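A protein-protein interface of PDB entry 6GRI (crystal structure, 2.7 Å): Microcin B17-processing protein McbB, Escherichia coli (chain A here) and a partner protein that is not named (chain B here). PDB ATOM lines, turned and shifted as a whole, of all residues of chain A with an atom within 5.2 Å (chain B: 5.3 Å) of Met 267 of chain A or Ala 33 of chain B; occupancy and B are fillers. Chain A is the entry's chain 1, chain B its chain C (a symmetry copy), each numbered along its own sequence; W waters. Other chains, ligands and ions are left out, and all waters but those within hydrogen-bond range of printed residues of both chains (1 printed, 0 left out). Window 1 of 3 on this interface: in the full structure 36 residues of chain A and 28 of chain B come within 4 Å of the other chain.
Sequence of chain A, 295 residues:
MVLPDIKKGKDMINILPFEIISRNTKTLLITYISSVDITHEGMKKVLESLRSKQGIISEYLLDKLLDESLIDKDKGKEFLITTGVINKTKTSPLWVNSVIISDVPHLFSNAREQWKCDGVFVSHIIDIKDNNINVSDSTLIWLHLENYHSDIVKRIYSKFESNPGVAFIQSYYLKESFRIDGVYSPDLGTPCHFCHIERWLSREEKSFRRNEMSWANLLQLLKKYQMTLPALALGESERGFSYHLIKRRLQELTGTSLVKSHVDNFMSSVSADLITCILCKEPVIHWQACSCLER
O of Val 263 of chain A sits at hydrogen-bond distance from N of Ala 33 of chain B (2.8 Å).
The backbone carbonyl oxygen (O) of Met 267 of chain A lies within hydrogen-bond range of the backbone NH (N) of Val 183 of chain A (3.0 Å). The guanidinium group (NH2) of Arg 249 of chain A lies within hydrogen-bond range of the backbone carbonyl oxygen (O) of Phe 266 of chain A. The backbone carbonyl oxygen (O) of Phe 38 of chain B lies within hydrogen-bond range of the side-chain hydroxyl (OG1) of Thr 42 of chain B, 2.7 Å away.
CD2 of Leu 188 of chain A touches CD1 of Leu 35 of chain B, at 3.6 Å. O of Asn 31 of chain B touches O of Val 263 of chain A, 3.9 Å away. Phe 32 of chain B touches Val 263 of chain A. Thr 42 of chain B touches Val 263 of chain A (OG1 to CG1, 3.6 Å). CA of Asp 264 of chain A touches O of Asn 31 of chain B, 3.3 Å away. Phe 266 of chain A touches Phe 38 of chain B (CE2 to CD1, 3.4 Å). CG2 of Thr 42 of chain B touches CG of Phe 266 of chain A (3.7 Å). CB of Ala 33 of chain B touches CG of Met 267 of chain A, at 3.4 Å.
Met 267 of chain A touches just one residue of chain B: Ala 33 (3.4 Å). Of chain A, only Val 263 and Met 267 come within 4 Å of Ala 33 of chain B. Of the printed residues of chain A, Thr 42 of chain B touches Val 263 and Phe 266. Printed residues of chain A within 4 Å of Leu 35 of chain B: Leu 188 (3.6 Å). Val 183 of chain A touches none of the printed residues of chain B. The nearest residue of chain B that does not touch Met 267 of chain A is Phe 38 of chain B (4.4 Å). The nearest printed residue of chain A that does not touch Phe 32 of chain B is Asp 264 of chain A (4.1 Å).
Printed residues of chain B that touch a printed residue of chain A: Asn 31, Phe 32, Ala 33, Leu 35, Phe 38 and Thr 42. Of the 14 printed residues of chain A, 5 touch a printed residue of chain B. Hydrophobic or aromatic side chains of chain A within 4 Å of the printed part of chain B: Leu 188, Val 263, Phe 266 and Met 267.
Water W1 lies within hydrogen-bond range of the backbone carbonyl oxygen (O) of Asp 264 of chain A and the backbone carbonyl oxygen (O) of Asn 31 of chain B.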
ATOM      1  N   TRP A  95     -36.850 -25.606  24.625  1.00  0.00           N
ATOM      2  CA  TRP A  95     -38.199 -25.700  24.089  1.00  0.00           C
ATOM      3  C   TRP A  95     -38.866 -27.020  24.482  1.00  0.00           C
ATOM      4  O   TRP A  95     -38.490 -28.093  24.008  1.00  0.00           O
ATOM      5  CB  TRP A  95     -38.171 -25.509  22.578  1.00  0.00           C
ATOM      6  CG  TRP A  95     -37.434 -24.264  22.180  1.00  0.00           C
ATOM      7  CD1 TRP A  95     -37.769 -22.979  22.485  1.00  0.00           C
ATOM      8  CD2 TRP A  95     -36.216 -24.194  21.432  1.00  0.00           C
ATOM      9  NE1 TRP A  95     -36.844 -22.110  21.959  1.00  0.00           N
ATOM     10  CE2 TRP A  95     -35.881 -22.831  21.307  1.00  0.00           C
ATOM     11  CE3 TRP A  95     -35.384 -25.151  20.845  1.00  0.00           C
ATOM     12  CZ2 TRP A  95     -34.745 -22.401  20.624  1.00  0.00           C
ATOM     13  CZ3 TRP A  95     -34.251 -24.727  20.159  1.00  0.00           C
ATOM     14  CH2 TRP A  95     -33.939 -23.364  20.058  1.00  0.00           C
ATOM     15  N   GLY A 182     -32.175 -19.987  10.022  1.00  0.00           N
ATOM     16  CA  GLY A 182     -31.786 -20.030  11.412  1.00  0.00           C
ATOM     17  C   GLY A 182     -32.964 -19.814  12.359  1.00  0.00           C
ATOM     18  O   GLY A 182     -34.041 -19.358  11.971  1.00  0.00           O
ATOM     19  N   VAL A 183     -32.735 -20.157  13.615  1.00  0.00           N
ATOM     20  CA  VAL A 183     -33.744 -20.121  14.646  1.00  0.00           C
ATOM     21  C   VAL A 183     -33.977 -18.670  15.037  1.00  0.00           C
ATOM     22  O   VAL A 183     -33.044 -17.975  15.446  1.00  0.00           O
ATOM     23  CB  VAL A 183     -33.296 -20.968  15.851  1.00  0.00           C
ATOM     24  CG1 VAL A 183     -34.204 -20.766  17.058  1.00  0.00           C
ATOM     25  CG2 VAL A 183     -33.270 -22.434  15.447  1.00  0.00           C
ATOM     26  N   LEU A 188     -33.541 -14.720  22.542  1.00  0.00           N
ATOM     27  CA  LEU A 188     -32.091 -14.765  22.257  1.00  0.00           C
ATOM     28  C   LEU A 188     -31.605 -13.645  21.300  1.00  0.00           C
ATOM     29  O   LEU A 188     -30.396 -13.375  21.208  1.00  0.00           O
ATOM     30  CB  LEU A 188     -31.699 -16.145  21.715  1.00  0.00           C
ATOM     31  CG  LEU A 188     -32.030 -17.311  22.655  1.00  0.00           C
ATOM     32  CD1 LEU A 188     -32.006 -18.630  21.906  1.00  0.00           C
ATOM     33  CD2 LEU A 188     -31.085 -17.349  23.849  1.00  0.00           C
ATOM     34  N   THR A 190     -32.124 -13.284  17.868  1.00  0.00           N
ATOM     35  CA  THR A 190     -31.573 -13.799  16.616  1.00  0.00           C
ATOM     36  C   THR A 190     -32.333 -13.311  15.382  1.00  0.00           C
ATOM     37  O   THR A 190     -33.478 -12.905  15.475  1.00  0.00           O
ATOM     38  CB  THR A 190     -31.563 -15.329  16.614  1.00  0.00           C
ATOM     39  OG1 THR A 190     -32.883 -15.814  16.852  1.00  0.00           O
ATOM     40  CG2 THR A 190     -30.628 -15.860  17.711  1.00  0.00           C
ATOM     41  N   ARG A 249     -32.663 -31.506  11.617  1.00  0.00           N
ATOM     42  CA  ARG A 249     -32.534 -30.181  12.216  1.00  0.00           C
ATOM     43  C   ARG A 249     -33.323 -30.070  13.529  1.00  0.00           C
ATOM     44  O   ARG A 249     -32.820 -29.486  14.501  1.00  0.00           O
ATOM     45  CB  ARG A 249     -32.971 -29.109  11.220  1.00  0.00           C
ATOM     46  CG  ARG A 249     -32.671 -27.686  11.652  1.00  0.00           C
ATOM     47  CD  ARG A 249     -31.187 -27.375  11.682  1.00  0.00           C
ATOM     48  NE  ARG A 249     -30.982 -26.022  12.184  1.00  0.00           N
ATOM     49  CZ  ARG A 249     -30.444 -25.674  13.358  1.00  0.00           C
ATOM     50  NH1 ARG A 249     -29.992 -26.562  14.241  1.00  0.00           N
ATOM     51  NH2 ARG A 249     -30.345 -24.377  13.650  1.00  0.00           N
ATOM     52  N   LEU A 253     -31.744 -29.725  17.427  1.00  0.00           N
ATOM     53  CA  LEU A 253     -32.242 -28.677  18.306  1.00  0.00           C
ATOM     54  C   LEU A 253     -32.924 -29.232  19.538  1.00  0.00           C
ATOM     55  O   LEU A 253     -32.634 -28.779  20.639  1.00  0.00           O
ATOM     56  CB  LEU A 253     -33.193 -27.738  17.549  1.00  0.00           C
ATOM     57  CG  LEU A 253     -32.497 -26.877  16.483  1.00  0.00           C
ATOM     58  CD1 LEU A 253     -33.485 -26.353  15.449  1.00  0.00           C
ATOM     59  CD2 LEU A 253     -31.722 -25.726  17.117  1.00  0.00           C
ATOM     60  N   VAL A 263     -20.781 -24.597  18.817  1.00  0.00           N
ATOM     61  CA  VAL A 263     -21.570 -23.451  19.266  1.00  0.00           C
ATOM     62  C   VAL A 263     -21.640 -22.293  18.266  1.00  0.00           C
ATOM     63  O   VAL A 263     -22.574 -21.479  18.348  1.00  0.00           O
ATOM     64  CB  VAL A 263     -21.113 -22.920  20.648  1.00  0.00           C
ATOM     65  CG1 VAL A 263     -21.429 -23.945  21.730  1.00  0.00           C
ATOM     66  CG2 VAL A 263     -19.631 -22.534  20.658  1.00  0.00           C
ATOM     67  N   ASP A 264     -20.697 -22.224  17.326  1.00  0.00           N
ATOM     68  CA  ASP A 264     -20.686 -21.150  16.329  1.00  0.00           C
ATOM     69  C   ASP A 264     -21.592 -21.375  15.110  1.00  0.00           C
ATOM     70  O   ASP A 264     -21.698 -20.482  14.265  1.00  0.00           O
ATOM     71  CB  ASP A 264     -19.253 -20.771  15.909  1.00  0.00           C
ATOM     72  CG  ASP A 264     -18.565 -21.817  15.022  1.00  0.00           C
ATOM     73  OD1 ASP A 264     -19.216 -22.774  14.549  1.00  0.00           O
ATOM     74  OD2 ASP A 264     -17.340 -21.667  14.802  1.00  0.00           O
ATOM     75  N   ASN A 265     -22.245 -22.535  15.014  1.00  0.00           N
ATOM     76  CA  ASN A 265     -23.232 -22.760  13.951  1.00  0.00           C
ATOM     77  C   ASN A 265     -24.461 -23.542  14.365  1.00  0.00           C
ATOM     78  O   ASN A 265     -25.147 -24.111  13.518  1.00  0.00           O
ATOM     79  CB  ASN A 265     -22.566 -23.413  12.724  1.00  0.00           C
ATOM     80  CG  ASN A 265     -22.519 -22.483  11.514  1.00  0.00           C
ATOM     81  OD1 ASN A 265     -23.078 -21.369  11.518  1.00  0.00           O
ATOM     82  ND2 ASN A 265     -21.836 -22.934  10.465  1.00  0.00           N
ATOM     83  N   PHE A 266     -24.782 -23.508  15.652  1.00  0.00           N
ATOM     84  CA  PHE A 266     -25.864 -24.320  16.193  1.00  0.00           C
ATOM     85  C   PHE A 266     -27.223 -23.753  15.801  1.00  0.00           C
ATOM     86  O   PHE A 266     -28.137 -24.502  15.471  1.00  0.00           O
ATOM     87  CB  PHE A 266     -25.718 -24.431  17.709  1.00  0.00           C
ATOM     88  CG  PHE A 266     -26.797 -25.230  18.363  1.00  0.00           C
ATOM     89  CD1 PHE A 266     -26.950 -26.581  18.074  1.00  0.00           C
ATOM     90  CD2 PHE A 266     -27.671 -24.637  19.276  1.00  0.00           C
ATOM     91  CE1 PHE A 266     -27.956 -27.321  18.679  1.00  0.00           C
ATOM     92  CE2 PHE A 266     -28.672 -25.375  19.882  1.00  0.00           C
ATOM     93  CZ  PHE A 266     -28.817 -26.717  19.581  1.00  0.00           C
ATOM     94  N   MET A 267     -27.326 -22.430  15.824  1.00  0.00           N
ATOM     95  CA  MET A 267     -28.561 -21.692  15.548  1.00  0.00           C
ATOM     96  C   MET A 267     -28.746 -21.329  14.070  1.00  0.00           C
ATOM     97  O   MET A 267     -29.797 -20.780  13.691  1.00  0.00           O
ATOM     98  CB  MET A 267     -28.529 -20.359  16.304  1.00  0.00           C
ATOM     99  CG  MET A 267     -28.380 -20.450  17.806  1.00  0.00           C
ATOM    100  SD  MET A 267     -29.951 -20.190  18.626  1.00  0.00           S
ATOM    101  CE  MET A 267     -30.730 -21.763  18.294  1.00  0.00           C
ATOM    102  N   SER A 268     -27.736 -21.612  13.246  1.00  0.00           N
ATOM    103  CA  SER A 268     -27.616 -21.002  11.929  1.00  0.00           C
ATOM    104  C   SER A 268     -28.469 -21.626  10.824  1.00  0.00           C
ATOM    105  O   SER A 268     -29.044 -22.710  10.978  1.00  0.00           O
ATOM    106  CB  SER A 268     -26.153 -21.006  11.525  1.00  0.00           C
ATOM    107  OG  SER A 268     -25.398 -20.341  12.515  1.00  0.00           O
ATOM    108  N   SER A 269     -28.551 -20.915   9.703  1.00  0.00           N
ATOM    109  CA  SER A 269     -29.323 -21.374   8.556  1.00  0.00           C
ATOM    110  C   SER A 269     -28.647 -22.591   7.926  1.00  0.00           C
ATOM    111  O   SER A 269     -27.447 -22.780   8.074  1.00  0.00           O
ATOM    112  CB  SER A 269     -29.470 -20.250   7.530  1.00  0.00           C
ATOM    113  OG  SER A 269     -28.238 -19.967   6.869  1.00  0.00           O
ATOM    114  N   ASN B  31     -19.771 -15.843  16.519  1.00  0.00           N
ATOM    115  CA  ASN B  31     -20.761 -15.737  17.589  1.00  0.00           C
ATOM    116  C   ASN B  31     -21.077 -17.131  18.051  1.00  0.00           C
ATOM    117  O   ASN B  31     -21.114 -18.050  17.246  1.00  0.00           O
ATOM    118  CB  ASN B  31     -22.051 -15.044  17.130  1.00  0.00           C
ATOM    119  CG  ASN B  31     -21.921 -13.538  17.051  1.00  0.00           C
ATOM    120  OD1 ASN B  31     -21.035 -12.946  17.651  1.00  0.00           O
ATOM    121  ND2 ASN B  31     -22.819 -12.913  16.315  1.00  0.00           N
ATOM    122  N   PHE B  32     -21.326 -17.266  19.344  1.00  0.00           N
ATOM    123  CA  PHE B  32     -21.610 -18.540  19.984  1.00  0.00           C
ATOM    124  C   PHE B  32     -23.081 -18.634  20.371  1.00  0.00           C
ATOM    125  O   PHE B  32     -23.737 -17.623  20.648  1.00  0.00           O
ATOM    126  CB  PHE B  32     -20.743 -18.678  21.248  1.00  0.00           C
ATOM    127  CG  PHE B  32     -19.352 -19.204  21.006  1.00  0.00           C
ATOM    128  CD1 PHE B  32     -18.787 -19.294  19.718  1.00  0.00           C
ATOM    129  CD2 PHE B  32     -18.590 -19.598  22.085  1.00  0.00           C
ATOM    130  CE1 PHE B  32     -17.510 -19.788  19.529  1.00  0.00           C
ATOM    131  CE2 PHE B  32     -17.303 -20.084  21.903  1.00  0.00           C
ATOM    132  CZ  PHE B  32     -16.764 -20.184  20.627  1.00  0.00           C
ATOM    133  N   ALA B  33     -23.585 -19.864  20.341  1.00  0.00           N
ATOM    134  CA  ALA B  33     -24.864 -20.226  20.908  1.00  0.00           C
ATOM    135  C   ALA B  33     -24.497 -21.092  22.099  1.00  0.00           C
ATOM    136  O   ALA B  33     -24.277 -22.303  21.979  1.00  0.00           O
ATOM    137  CB  ALA B  33     -25.699 -20.990  19.892  1.00  0.00           C
ATOM    138  N   SER B  34     -24.417 -20.437  23.248  1.00  0.00           N
ATOM    139  CA  SER B  34     -23.824 -20.982  24.453  1.00  0.00           C
ATOM    140  C   SER B  34     -24.805 -20.866  25.619  1.00  0.00           C
ATOM    141  O   SER B  34     -24.812 -19.868  26.322  1.00  0.00           O
ATOM    142  CB  SER B  34     -22.550 -20.184  24.729  1.00  0.00           C
ATOM    143  OG  SER B  34     -21.927 -20.578  25.925  1.00  0.00           O
ATOM    144  N   LEU B  35     -25.644 -21.881  25.810  1.00  0.00           N
ATOM    145  CA  LEU B  35     -26.610 -21.917  26.923  1.00  0.00           C
ATOM    146  C   LEU B  35     -26.591 -23.260  27.642  1.00  0.00           C
ATOM    147  O   LEU B  35     -26.286 -24.282  27.028  1.00  0.00           O
ATOM    148  CB  LEU B  35     -28.035 -21.694  26.416  1.00  0.00           C
ATOM    149  CG  LEU B  35     -28.352 -20.413  25.637  1.00  0.00           C
ATOM    150  CD1 LEU B  35     -29.738 -20.512  25.000  1.00  0.00           C
ATOM    151  CD2 LEU B  35     -28.246 -19.183  26.535  1.00  0.00           C
ATOM    152  N   PHE B  38     -28.229 -26.170  25.909  1.00  0.00           N
ATOM    153  CA  PHE B  38     -27.500 -26.716  24.767  1.00  0.00           C
ATOM    154  C   PHE B  38     -26.181 -27.423  25.138  1.00  0.00           C
ATOM    155  O   PHE B  38     -25.479 -27.900  24.251  1.00  0.00           O
ATOM    156  CB  PHE B  38     -27.207 -25.601  23.754  1.00  0.00           C
ATOM    157  CG  PHE B  38     -28.424 -24.832  23.294  1.00  0.00           C
ATOM    158  CD1 PHE B  38     -29.671 -25.435  23.166  1.00  0.00           C
ATOM    159  CD2 PHE B  38     -28.299 -23.495  22.932  1.00  0.00           C
ATOM    160  CE1 PHE B  38     -30.766 -24.707  22.721  1.00  0.00           C
ATOM    161  CE2 PHE B  38     -29.393 -22.767  22.487  1.00  0.00           C
ATOM    162  CZ  PHE B  38     -30.628 -23.371  22.386  1.00  0.00           C
ATOM    163  N   THR B  42     -24.007 -29.396  22.209  1.00  0.00           N
ATOM    164  CA  THR B  42     -23.026 -28.563  21.545  1.00  0.00           C
ATOM    165  C   THR B  42     -21.652 -28.861  22.144  1.00  0.00           C
ATOM    166  O   THR B  42     -21.549 -29.561  23.151  1.00  0.00           O
ATOM    167  CB  THR B  42     -23.358 -27.046  21.687  1.00  0.00           C
ATOM    168  OG1 THR B  42     -23.378 -26.659  23.064  1.00  0.00           O
ATOM    169  CG2 THR B  42     -24.708 -26.716  21.090  1.00  0.00           C
ATOM    170  N   THR B 239     -23.651 -16.380  24.709  1.00  0.00           N
ATOM    171  CA  THR B 239     -24.423 -16.223  23.489  1.00  0.00           C
ATOM    172  C   THR B 239     -24.436 -14.730  23.120  1.00  0.00           C
ATOM    173  O   THR B 239     -25.094 -13.931  23.776  1.00  0.00           O
ATOM    174  CB  THR B 239     -25.865 -16.740  23.688  1.00  0.00           C
ATOM    175  OG1 THR B 239     -25.846 -18.068  24.209  1.00  0.00           O
ATOM    176  CG2 THR B 239     -26.639 -16.732  22.394  1.00  0.00           C
HETATM  177  O   HOH W   1     -22.456 -17.851  14.339  1.00  0.00           O
